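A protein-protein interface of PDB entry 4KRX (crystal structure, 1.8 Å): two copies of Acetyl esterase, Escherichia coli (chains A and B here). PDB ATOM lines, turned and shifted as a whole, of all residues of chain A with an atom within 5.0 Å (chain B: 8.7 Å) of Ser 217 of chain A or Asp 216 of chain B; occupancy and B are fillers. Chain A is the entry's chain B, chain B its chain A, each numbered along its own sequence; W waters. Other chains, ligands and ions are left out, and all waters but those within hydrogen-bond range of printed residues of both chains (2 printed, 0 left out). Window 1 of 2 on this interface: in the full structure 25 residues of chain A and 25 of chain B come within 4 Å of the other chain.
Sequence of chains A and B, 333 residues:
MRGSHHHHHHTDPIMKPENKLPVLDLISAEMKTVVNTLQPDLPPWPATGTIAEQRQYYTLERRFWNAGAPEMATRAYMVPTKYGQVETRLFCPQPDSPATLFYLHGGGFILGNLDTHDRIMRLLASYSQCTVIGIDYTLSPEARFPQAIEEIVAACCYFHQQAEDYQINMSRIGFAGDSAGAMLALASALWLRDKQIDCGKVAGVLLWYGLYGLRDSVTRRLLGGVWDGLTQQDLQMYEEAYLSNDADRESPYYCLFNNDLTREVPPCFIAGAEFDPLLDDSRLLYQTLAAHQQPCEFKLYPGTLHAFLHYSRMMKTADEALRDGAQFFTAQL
The backbone NH (N) of Arg 215 of chain B sits at hydrogen-bond distance from the side-chain carboxylate (OD2) of Asp 216 of chain A (2.8 Å). N of Arg 215 of chain A is in hydrogen-bond range of OD2 of Asp 216 of chain B (2.9 Å). The backbone carbonyl oxygen (O) of Asp 216 of chain A sits close to the backbone carbonyl oxygen (O) of Asp 216 of chain B, at 3.1 Å.
The side-chain carboxylate (OD2) of Asp 281 of chain B lies within hydrogen-bond range of the backbone NH (N) of Leu 214 of chain B (3.2 Å). The side-chain hydroxyl (OG) of Ser 217 of chain B lies within hydrogen-bond range of the side-chain hydroxyl (OG1) of Thr 219 of chain B. OG of Ser 217 of chain B is in hydrogen-bond range of N of Arg 220 of chain B (2.9 Å). N of Val 218 of chain B sits at hydrogen-bond distance from OD2 of Asp 280 of chain B (3.4 Å). The backbone carbonyl oxygen (O) of Leu 214 of chain A is in hydrogen-bond range of the guanidinium group (NH2) of Arg 220 of chain A (2.9 Å). The side-chain carboxylate (OD2) of Asp 280 of chain A is in hydrogen-bond range of the backbone NH (N) of Val 218 of chain A, at 3.4 Å.
NH2 of Arg 221 of chain B touches O of Gly 213 of chain A, at 3.9 Å. Asp 216 of chain B touches Leu 214 of chain A. CD2 of Leu 214 of chain A touches CG of Arg 221 of chain B, at 3.8 Å. Leu 214 of chain B touches Asp 216 of chain A. N of Ser 217 of chain B touches O of Asp 216 of chain A (3.6 Å). Ser 217 of chain A touches Leu 214 of chain B. Asp 216 of chain B touches Ser 217 of chain A (O to N, 3.7 Å). CG2 of Val 218 of chain A touches O of Asp 280 of chain B (3.6 Å). Arg 221 of chain A touches Leu 214 of chain B (CG to CD2, 3.8 Å). CD2 of Leu 284 of chain B touches CB of Arg 221 of chain A, at 3.6 Å.
Of chain B, only Leu 214, Arg 215, Asp 216 and Ser 217 come within 4 Å of Asp 216 of chain A. Printed residues of chain B within 4 Å of Val 218 of chain A: Asp 280 (3.6 Å) and Leu 284 (3.7 Å). Of the printed residues of chain A, Gly 213 of chain B touches Arg 221. Asp 216 of chain B touches just these residues of chain A: Leu 214 (3.5 Å), Arg 215 (2.9 Å), Asp 216 (3.1 Å) and Ser 217 (3.7 Å). Printed residues of chain A within 4 Å of Ser 217 of chain B: Leu 214 (3.9 Å) and Asp 216 (3.6 Å). Gln 232 of chain B touches none of the printed residues of chain A. Asp 281 of chain B touches none of the printed residues of chain A. The nearest printed residue of chain A that does not touch Gly 213 of chain B is Asp 216 of chain A (4.1 Å).
Printed residues of chain A that touch a printed residue of chain B: Gly 213, Leu 214, Arg 215, Asp 216, Ser 217, Val 218, Arg 221 and Asp 280. Among the printed residues, 17 pairs touch across the chains.
Gly 213 of chain A touches Arg 221 of chain B, and with the chains exchanged Arg 221 of chain A touches Gly 213 of chain B. Leu 214 of chain A touches Arg 221 of chain B, and with the chains exchanged Arg 221 of chain A touches Leu 214 of chain B. Arg 215 of chain A touches Asp 216 of chain B, and with the chains exchanged Asp 216 of chain A touches Arg 215 of chain B. Val 218 of chain A touches Asp 280 of chain B, and with the chains exchanged Asp 280 of chain A touches Val 218 of chain B. Of the 17 pairs that touch across the chains among the printed residues, 15 have their exchanged pair printed and touching as well.
Water W2 lies within hydrogen-bond range of the side-chain carboxylate of Asp 280 of chain B (2.7 Å), the side-chain carboxylate of Asp 280 of chain A (2.7 Å), the backbone NH of Val 218 of chain A (3.1 Å) and the backbone NH of Val 218 of chain B (3.1 Å). Water W1 bridges the backbone carbonyl oxygen of Phe 257 of chain B and the guanidinium group of Arg 221 of chain A.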
ATOM      1  N   GLY A 213       2.779  -8.777  -1.060  1.00  0.00           N
ATOM      2  CA  GLY A 213       2.311  -8.041   0.140  1.00  0.00           C
ATOM      3  C   GLY A 213       1.417  -8.697   1.183  1.00  0.00           C
ATOM      4  O   GLY A 213       0.981  -8.017   2.085  1.00  0.00           O
ATOM      5  N   LEU A 214       1.076  -9.979   1.055  1.00  0.00           N
ATOM      6  CA  LEU A 214       0.347 -10.674   2.132  1.00  0.00           C
ATOM      7  C   LEU A 214       1.183 -10.643   3.373  1.00  0.00           C
ATOM      8  O   LEU A 214       2.365 -10.902   3.303  1.00  0.00           O
ATOM      9  CB  LEU A 214       0.094 -12.161   1.812  1.00  0.00           C
ATOM     10  CG  LEU A 214      -1.112 -12.461   0.949  1.00  0.00           C
ATOM     11  CD1 LEU A 214      -1.126 -13.929   0.574  1.00  0.00           C
ATOM     12  CD2 LEU A 214      -2.400 -12.102   1.676  1.00  0.00           C
ATOM     13  N   ARG A 215       0.564 -10.412   4.508  1.00  0.00           N
ATOM     14  CA  ARG A 215       1.301 -10.344   5.780  1.00  0.00           C
ATOM     15  C   ARG A 215       1.270 -11.674   6.486  1.00  0.00           C
ATOM     16  O   ARG A 215       2.011 -11.887   7.472  1.00  0.00           O
ATOM     17  CB  ARG A 215       0.651  -9.268   6.664  1.00  0.00           C
ATOM     18  CG  ARG A 215       0.647  -7.892   6.012  1.00  0.00           C
ATOM     19  CD  ARG A 215       0.889  -6.730   6.962  1.00  0.00           C
ATOM     20  NE  ARG A 215       2.197  -6.764   7.687  1.00  0.00           N
ATOM     21  CZ  ARG A 215       3.425  -6.612   7.149  1.00  0.00           C
ATOM     22  NH1 ARG A 215       3.635  -6.430   5.814  1.00  0.00           N
ATOM     23  NH2 ARG A 215       4.483  -6.679   7.956  1.00  0.00           N
ATOM     24  N   ASP A 216       0.399 -12.580   6.040  1.00  0.00           N
ATOM     25  CA  ASP A 216       0.170 -13.896   6.689  1.00  0.00           C
ATOM     26  C   ASP A 216      -0.635 -14.713   5.678  1.00  0.00           C
ATOM     27  O   ASP A 216      -1.280 -14.123   4.753  1.00  0.00           O
ATOM     28  CB  ASP A 216      -0.593 -13.682   8.018  1.00  0.00           C
ATOM     29  CG  ASP A 216      -0.439 -14.821   9.037  1.00  0.00           C
ATOM     30  OD1 ASP A 216       0.231 -15.813   8.683  1.00  0.00           O
ATOM     31  OD2 ASP A 216      -1.139 -14.720  10.115  1.00  0.00           O
ATOM     32  N   SER A 217      -0.657 -16.009   5.807  1.00  0.00           N
ATOM     33  CA  SER A 217      -1.400 -16.875   4.909  1.00  0.00           C
ATOM     34  C   SER A 217      -1.285 -18.298   5.399  1.00  0.00           C
ATOM     35  O   SER A 217      -0.401 -18.619   6.223  1.00  0.00           O
ATOM     36  CB  SER A 217      -0.841 -16.836   3.462  1.00  0.00           C
ATOM     37  OG  SER A 217       0.474 -17.392   3.411  1.00  0.00           O
ATOM     38  N   VAL A 218      -2.077 -19.156   4.771  1.00  0.00           N
ATOM     39  CA  VAL A 218      -2.095 -20.542   5.027  1.00  0.00           C
ATOM     40  C   VAL A 218      -0.668 -21.083   4.776  1.00  0.00           C
ATOM     41  O   VAL A 218      -0.096 -21.797   5.612  1.00  0.00           O
ATOM     42  CB  VAL A 218      -3.128 -21.335   4.203  1.00  0.00           C
ATOM     43  CG1 VAL A 218      -2.917 -22.856   4.360  1.00  0.00           C
ATOM     44  CG2 VAL A 218      -4.563 -20.975   4.599  1.00  0.00           C
ATOM     45  N   THR A 219      -0.101 -20.739   3.645  1.00  0.00           N
ATOM     46  CA  THR A 219       1.220 -21.254   3.318  1.00  0.00           C
ATOM     47  C   THR A 219       2.339 -20.648   4.161  1.00  0.00           C
ATOM     48  O   THR A 219       3.284 -21.338   4.427  1.00  0.00           O
ATOM     49  CB  THR A 219       1.523 -21.170   1.779  1.00  0.00           C
ATOM     50  OG1 THR A 219       1.373 -19.836   1.228  1.00  0.00           O
ATOM     51  CG2 THR A 219       0.621 -22.098   1.056  1.00  0.00           C
ATOM     52  N   ARG A 220       2.221 -19.366   4.559  1.00  0.00           N
ATOM     53  CA  ARG A 220       3.222 -18.726   5.401  1.00  0.00           C
ATOM     54  C   ARG A 220       3.250 -19.468   6.734  1.00  0.00           C
ATOM     55  O   ARG A 220       4.325 -19.650   7.335  1.00  0.00           O
ATOM     56  CB  ARG A 220       2.994 -17.230   5.563  1.00  0.00           C
ATOM     57  CG  ARG A 220       3.549 -16.391   4.423  1.00  0.00           C
ATOM     58  CD  ARG A 220       2.925 -15.019   4.372  1.00  0.00           C
ATOM     59  NE  ARG A 220       3.212 -14.285   3.123  1.00  0.00           N
ATOM     60  CZ  ARG A 220       4.069 -13.285   3.007  1.00  0.00           C
ATOM     61  NH1 ARG A 220       4.827 -12.950   4.047  1.00  0.00           N
ATOM     62  NH2 ARG A 220       4.171 -12.622   1.857  1.00  0.00           N
ATOM     63  N   ARG A 221       2.093 -19.953   7.173  1.00  0.00           N
ATOM     64  CA  ARG A 221       2.050 -20.662   8.469  1.00  0.00           C
ATOM     65  C   ARG A 221       2.589 -22.084   8.362  1.00  0.00           C
ATOM     66  O   ARG A 221       3.231 -22.592   9.304  1.00  0.00           O
ATOM     67  CB  ARG A 221       0.637 -20.657   9.021  1.00  0.00           C
ATOM     68  CG  ARG A 221       0.181 -19.290   9.473  1.00  0.00           C
ATOM     69  CD  ARG A 221       0.727 -18.869  10.837  1.00  0.00           C
ATOM     70  NE  ARG A 221       0.238 -17.529  11.149  1.00  0.00           N
ATOM     71  CZ  ARG A 221       0.304 -16.949  12.339  1.00  0.00           C
ATOM     72  NH1 ARG A 221       0.911 -17.555  13.332  1.00  0.00           N
ATOM     73  NH2 ARG A 221      -0.213 -15.741  12.491  1.00  0.00           N
ATOM     74  N   PRO A 277       6.476 -20.870   1.409  1.00  0.00           N
ATOM     75  CA  PRO A 277       5.508 -20.152   2.242  1.00  0.00           C
ATOM     76  C   PRO A 277       4.838 -19.042   1.384  1.00  0.00           C
ATOM     77  O   PRO A 277       3.777 -18.586   1.726  1.00  0.00           O
ATOM     78  CB  PRO A 277       6.325 -19.515   3.308  1.00  0.00           C
ATOM     79  CG  PRO A 277       7.765 -19.660   2.878  1.00  0.00           C
ATOM     80  CD  PRO A 277       7.818 -20.875   2.027  1.00  0.00           C
ATOM     81  N   ASP A 280       0.933 -18.808  -1.453  1.00  0.00           N
ATOM     82  CA  ASP A 280      -0.397 -18.137  -1.445  1.00  0.00           C
ATOM     83  C   ASP A 280      -0.400 -16.750  -1.966  1.00  0.00           C
ATOM     84  O   ASP A 280      -1.465 -16.233  -2.472  1.00  0.00           O
ATOM     85  CB  ASP A 280      -0.963 -18.184  -0.003  1.00  0.00           C
ATOM     86  CG  ASP A 280      -1.782 -19.404   0.268  1.00  0.00           C
ATOM     87  OD1 ASP A 280      -1.971 -20.264  -0.630  1.00  0.00           O
ATOM     88  OD2 ASP A 280      -2.254 -19.552   1.420  1.00  0.00           O
ATOM     89  N   LYS B  20     -12.168  -7.181  -4.480  1.00  0.00           N
ATOM     90  CA  LYS B  20     -12.913  -8.292  -3.904  1.00  0.00           C
ATOM     91  C   LYS B  20     -13.749  -9.018  -4.908  1.00  0.00           C
ATOM     92  O   LYS B  20     -14.122  -8.442  -6.000  1.00  0.00           O
ATOM     93  CB  LYS B  20     -13.773  -7.778  -2.775  1.00  0.00           C
ATOM     94  CG  LYS B  20     -12.969  -7.102  -1.692  1.00  0.00           C
ATOM     95  CD  LYS B  20     -12.919  -7.920  -0.467  1.00  0.00           C
ATOM     96  CE  LYS B  20     -12.222  -7.261   0.713  1.00  0.00           C
ATOM     97  NZ  LYS B  20     -11.334  -8.311   1.314  1.00  0.00           N
ATOM     98  N   GLY B 213      -6.491 -17.047  14.315  1.00  0.00           N
ATOM     99  CA  GLY B 213      -5.372 -16.162  14.464  1.00  0.00           C
ATOM    100  C   GLY B 213      -4.617 -15.758  13.234  1.00  0.00           C
ATOM    101  O   GLY B 213      -3.649 -15.048  13.378  1.00  0.00           O
ATOM    102  N   LEU B 214      -5.058 -16.158  12.017  1.00  0.00           N
ATOM    103  CA  LEU B 214      -4.464 -15.594  10.832  1.00  0.00           C
ATOM    104  C   LEU B 214      -4.628 -14.093  10.861  1.00  0.00           C
ATOM    105  O   LEU B 214      -5.712 -13.586  11.154  1.00  0.00           O
ATOM    106  CB  LEU B 214      -5.134 -16.104   9.549  1.00  0.00           C
ATOM    107  CG  LEU B 214      -4.553 -17.446   9.132  1.00  0.00           C
ATOM    108  CD1 LEU B 214      -5.313 -18.054   7.991  1.00  0.00           C
ATOM    109  CD2 LEU B 214      -3.063 -17.362   8.779  1.00  0.00           C
ATOM    110  N   ARG B 215      -3.594 -13.380  10.446  1.00  0.00           N
ATOM    111  CA  ARG B 215      -3.705 -11.935  10.314  1.00  0.00           C
ATOM    112  C   ARG B 215      -4.043 -11.418   8.926  1.00  0.00           C
ATOM    113  O   ARG B 215      -4.312 -10.232   8.808  1.00  0.00           O
ATOM    114  CB  ARG B 215      -2.403 -11.297  10.794  1.00  0.00           C
ATOM    115  CG  ARG B 215      -2.138 -11.707  12.257  1.00  0.00           C
ATOM    116  CD  ARG B 215      -1.235 -10.728  13.004  1.00  0.00           C
ATOM    117  NE  ARG B 215      -1.872  -9.400  13.148  1.00  0.00           N
ATOM    118  CZ  ARG B 215      -2.834  -9.073  14.010  1.00  0.00           C
ATOM    119  NH1 ARG B 215      -3.329  -9.957  14.885  1.00  0.00           N
ATOM    120  NH2 ARG B 215      -3.316  -7.833  13.989  1.00  0.00           N
ATOM    121  N   ASP B 216      -4.049 -12.299   7.951  1.00  0.00           N
ATOM    122  CA  ASP B 216      -4.206 -11.952   6.500  1.00  0.00           C
ATOM    123  C   ASP B 216      -4.281 -13.310   5.849  1.00  0.00           C
ATOM    124  O   ASP B 216      -3.863 -14.315   6.465  1.00  0.00           O
ATOM    125  CB  ASP B 216      -2.959 -11.213   5.983  1.00  0.00           C
ATOM    126  CG  ASP B 216      -3.248 -10.339   4.739  1.00  0.00           C
ATOM    127  OD1 ASP B 216      -4.391 -10.403   4.288  1.00  0.00           O
ATOM    128  OD2 ASP B 216      -2.281  -9.700   4.248  1.00  0.00           O
ATOM    129  N   SER B 217      -4.796 -13.419   4.640  1.00  0.00           N
ATOM    130  CA  SER B 217      -4.895 -14.715   3.944  1.00  0.00           C
ATOM    131  C   SER B 217      -5.483 -14.425   2.590  1.00  0.00           C
ATOM    132  O   SER B 217      -5.998 -13.285   2.389  1.00  0.00           O
ATOM    133  CB  SER B 217      -5.883 -15.707   4.627  1.00  0.00           C
ATOM    134  OG  SER B 217      -7.223 -15.154   4.680  1.00  0.00           O
ATOM    135  N   VAL B 218      -5.419 -15.390   1.715  1.00  0.00           N
ATOM    136  CA  VAL B 218      -6.087 -15.305   0.389  1.00  0.00           C
ATOM    137  C   VAL B 218      -7.557 -14.955   0.541  1.00  0.00           C
ATOM    138  O   VAL B 218      -8.076 -14.015  -0.111  1.00  0.00           O
ATOM    139  CB  VAL B 218      -5.890 -16.644  -0.339  1.00  0.00           C
ATOM    140  CG1 VAL B 218      -6.694 -16.720  -1.621  1.00  0.00           C
ATOM    141  CG2 VAL B 218      -4.387 -16.887  -0.612  1.00  0.00           C
ATOM    142  N   THR B 219      -8.295 -15.699   1.357  1.00  0.00           N
ATOM    143  CA  THR B 219      -9.743 -15.452   1.591  1.00  0.00           C
ATOM    144  C   THR B 219     -10.032 -14.095   2.241  1.00  0.00           C
ATOM    145  O   THR B 219     -10.950 -13.370   1.766  1.00  0.00           O
ATOM    146  CB  THR B 219     -10.442 -16.609   2.260  1.00  0.00           C
ATOM    147  OG1 THR B 219      -9.782 -16.889   3.537  1.00  0.00           O
ATOM    148  CG2 THR B 219     -10.378 -17.847   1.325  1.00  0.00           C
ATOM    149  N   ARG B 220      -9.212 -13.610   3.163  1.00  0.00           N
ATOM    150  CA  ARG B 220      -9.425 -12.265   3.750  1.00  0.00           C
ATOM    151  C   ARG B 220      -9.283 -11.210   2.696  1.00  0.00           C
ATOM    152  O   ARG B 220     -10.018 -10.172   2.740  1.00  0.00           O
ATOM    153  CB  ARG B 220      -8.471 -11.998   4.893  1.00  0.00           C
ATOM    154  CG  ARG B 220      -8.961 -12.776   6.113  1.00  0.00           C
ATOM    155  CD  ARG B 220      -7.868 -12.764   7.180  1.00  0.00           C
ATOM    156  NE  ARG B 220      -8.182 -13.701   8.250  1.00  0.00           N
ATOM    157  CZ  ARG B 220      -8.297 -13.355   9.519  1.00  0.00           C
ATOM    158  NH1 ARG B 220      -8.179 -12.031   9.850  1.00  0.00           N
ATOM    159  NH2 ARG B 220      -8.508 -14.306  10.431  1.00  0.00           N
ATOM    160  N   ARG B 221      -8.376 -11.437   1.746  1.00  0.00           N
ATOM    161  CA  ARG B 221      -8.192 -10.419   0.676  1.00  0.00           C
ATOM    162  C   ARG B 221      -9.335 -10.448  -0.325  1.00  0.00           C
ATOM    163  O   ARG B 221      -9.776  -9.418  -0.810  1.00  0.00           O
ATOM    164  CB  ARG B 221      -6.847 -10.647  -0.026  1.00  0.00           C
ATOM    165  CG  ARG B 221      -5.658 -10.304   0.867  1.00  0.00           C
ATOM    166  CD  ARG B 221      -5.471  -8.772   0.949  1.00  0.00           C
ATOM    167  NE  ARG B 221      -4.397  -8.455   1.843  1.00  0.00           N
ATOM    168  CZ  ARG B 221      -3.730  -7.308   1.961  1.00  0.00           C
ATOM    169  NH1 ARG B 221      -4.057  -6.221   1.283  1.00  0.00           N
ATOM    170  NH2 ARG B 221      -2.767  -7.272   2.888  1.00  0.00           N
ATOM    171  N   LEU B 222      -9.767 -11.639  -0.726  1.00  0.00           N
ATOM    172  CA  LEU B 222     -10.839 -11.801  -1.701  1.00  0.00           C
ATOM    173  C   LEU B 222     -12.286 -11.507  -1.210  1.00  0.00           C
ATOM    174  O   LEU B 222     -13.187 -11.161  -2.054  1.00  0.00           O
ATOM    175  CB  LEU B 222     -10.776 -13.227  -2.197  1.00  0.00           C
ATOM    176  CG  LEU B 222      -9.623 -13.526  -3.167  1.00  0.00           C
ATOM    177  CD1 LEU B 222      -9.548 -15.004  -3.497  1.00  0.00           C
ATOM    178  CD2 LEU B 222      -9.795 -12.718  -4.457  1.00  0.00           C
ATOM    179  N   GLN B 232     -11.461  -6.022   6.364  1.00  0.00           N
ATOM    180  CA  GLN B 232     -10.233  -5.878   7.166  1.00  0.00           C
ATOM    181  C   GLN B 232     -10.456  -4.943   8.326  1.00  0.00           C
ATOM    182  O   GLN B 232      -9.978  -5.200   9.425  1.00  0.00           O
ATOM    183  CB  GLN B 232      -9.038  -5.378   6.319  1.00  0.00           C
ATOM    184  CG  GLN B 232      -7.673  -5.437   7.055  1.00  0.00           C
ATOM    185  CD  GLN B 232      -6.456  -5.219   6.111  1.00  0.00           C
ATOM    186  OE1 GLN B 232      -6.435  -4.266   5.316  1.00  0.00           O
ATOM    187  NE2 GLN B 232      -5.447  -6.113   6.194  1.00  0.00           N
ATOM    188  N   LEU B 235     -12.570  -6.337  11.048  1.00  0.00           N
ATOM    189  CA  LEU B 235     -11.837  -7.374  11.821  1.00  0.00           C
ATOM    190  C   LEU B 235     -10.897  -6.706  12.807  1.00  0.00           C
ATOM    191  O   LEU B 235     -10.765  -7.171  13.931  1.00  0.00           O
ATOM    192  CB  LEU B 235     -11.093  -8.333  10.880  1.00  0.00           C
ATOM    193  CG  LEU B 235     -12.085  -9.235  10.144  1.00  0.00           C
ATOM    194  CD1 LEU B 235     -11.353  -9.961   9.038  1.00  0.00           C
ATOM    195  CD2 LEU B 235     -12.775 -10.231  11.064  1.00  0.00           C
ATOM    196  N   PHE B 257      -2.771 -20.718  16.199  1.00  0.00           N
ATOM    197  CA  PHE B 257      -1.662 -21.280  15.426  1.00  0.00           C
ATOM    198  C   PHE B 257      -0.278 -21.111  16.052  1.00  0.00           C
ATOM    199  O   PHE B 257       0.668 -21.663  15.544  1.00  0.00           O
ATOM    200  CB  PHE B 257      -1.681 -20.696  14.021  1.00  0.00           C
ATOM    201  CG  PHE B 257      -3.013 -20.915  13.316  1.00  0.00           C
ATOM    202  CD1 PHE B 257      -3.431 -22.198  13.042  1.00  0.00           C
ATOM    203  CD2 PHE B 257      -3.812 -19.848  12.905  1.00  0.00           C
ATOM    204  CE1 PHE B 257      -4.608 -22.504  12.406  1.00  0.00           C
ATOM    205  CE2 PHE B 257      -5.023 -20.123  12.258  1.00  0.00           C
ATOM    206  CZ  PHE B 257      -5.415 -21.430  11.970  1.00  0.00           C
ATOM    207  N   PRO B 277     -14.418 -14.598   4.387  1.00  0.00           N
ATOM    208  CA  PRO B 277     -13.005 -14.296   4.400  1.00  0.00           C
ATOM    209  C   PRO B 277     -12.256 -15.110   5.454  1.00  0.00           C
ATOM    210  O   PRO B 277     -11.045 -15.190   5.339  1.00  0.00           O
ATOM    211  CB  PRO B 277     -12.954 -12.877   4.820  1.00  0.00           C
ATOM    212  CG  PRO B 277     -14.258 -12.541   5.468  1.00  0.00           C
ATOM    213  CD  PRO B 277     -15.261 -13.402   4.712  1.00  0.00           C
ATOM    214  N   LEU B 278     -12.980 -15.597   6.445  1.00  0.00           N
ATOM    215  CA  LEU B 278     -12.323 -16.438   7.498  1.00  0.00           C
ATOM    216  C   LEU B 278     -12.138 -17.865   7.092  1.00  0.00           C
ATOM    217  O   LEU B 278     -11.556 -18.687   7.909  1.00  0.00           O
ATOM    218  CB  LEU B 278     -13.143 -16.325   8.799  1.00  0.00           C
ATOM    219  CG  LEU B 278     -13.335 -14.888   9.302  1.00  0.00           C
ATOM    220  CD1 LEU B 278     -14.159 -14.862  10.578  1.00  0.00           C
ATOM    221  CD2 LEU B 278     -12.003 -14.200   9.549  1.00  0.00           C
ATOM    222  N   ASP B 280     -10.033 -19.442   5.221  1.00  0.00           N
ATOM    223  CA  ASP B 280      -8.610 -19.915   5.263  1.00  0.00           C
ATOM    224  C   ASP B 280      -8.182 -20.259   6.669  1.00  0.00           C
ATOM    225  O   ASP B 280      -7.297 -21.148   6.869  1.00  0.00           O
ATOM    226  CB  ASP B 280      -7.700 -18.900   4.601  1.00  0.00           C
ATOM    227  CG  ASP B 280      -7.547 -19.145   3.051  1.00  0.00           C
ATOM    228  OD1 ASP B 280      -8.085 -20.115   2.485  1.00  0.00           O
ATOM    229  OD2 ASP B 280      -6.741 -18.432   2.424  1.00  0.00           O
ATOM    230  N   ASP B 281      -8.792 -19.638   7.679  1.00  0.00           N
ATOM    231  CA  ASP B 281      -8.474 -20.015   9.075  1.00  0.00           C
ATOM    232  C   ASP B 281      -8.878 -21.494   9.359  1.00  0.00           C
ATOM    233  O   ASP B 281      -8.145 -22.272  10.034  1.00  0.00           O
ATOM    234  CB  ASP B 281      -9.178 -19.122  10.086  1.00  0.00           C
ATOM    235  CG  ASP B 281      -8.519 -17.786  10.268  1.00  0.00           C
ATOM    236  OD1 ASP B 281      -8.591 -16.933   9.329  1.00  0.00           O
ATOM    237  OD2 ASP B 281      -7.861 -17.617  11.339  1.00  0.00           O
ATOM    238  N   LEU B 284      -6.491 -23.749   7.263  1.00  0.00           N
ATOM    239  CA  LEU B 284      -5.159 -23.908   7.933  1.00  0.00           C
ATOM    240  C   LEU B 284      -5.301 -24.781   9.120  1.00  0.00           C
ATOM    241  O   LEU B 284      -4.358 -25.690   9.334  1.00  0.00           O
ATOM    242  CB  LEU B 284      -4.584 -22.567   8.298  1.00  0.00           C
ATOM    243  CG  LEU B 284      -3.290 -22.629   9.103  1.00  0.00           C
ATOM    244  CD1 LEU B 284      -2.194 -23.344   8.305  1.00  0.00           C
ATOM    245  CD2 LEU B 284      -2.902 -21.259   9.550  1.00  0.00           C
HETATM  246  O   HOH W   1       2.191 -20.203  13.540  1.00  0.00           O
HETATM  247  O   HOH W   2      -4.128 -18.052   2.725  1.00  0.00           O
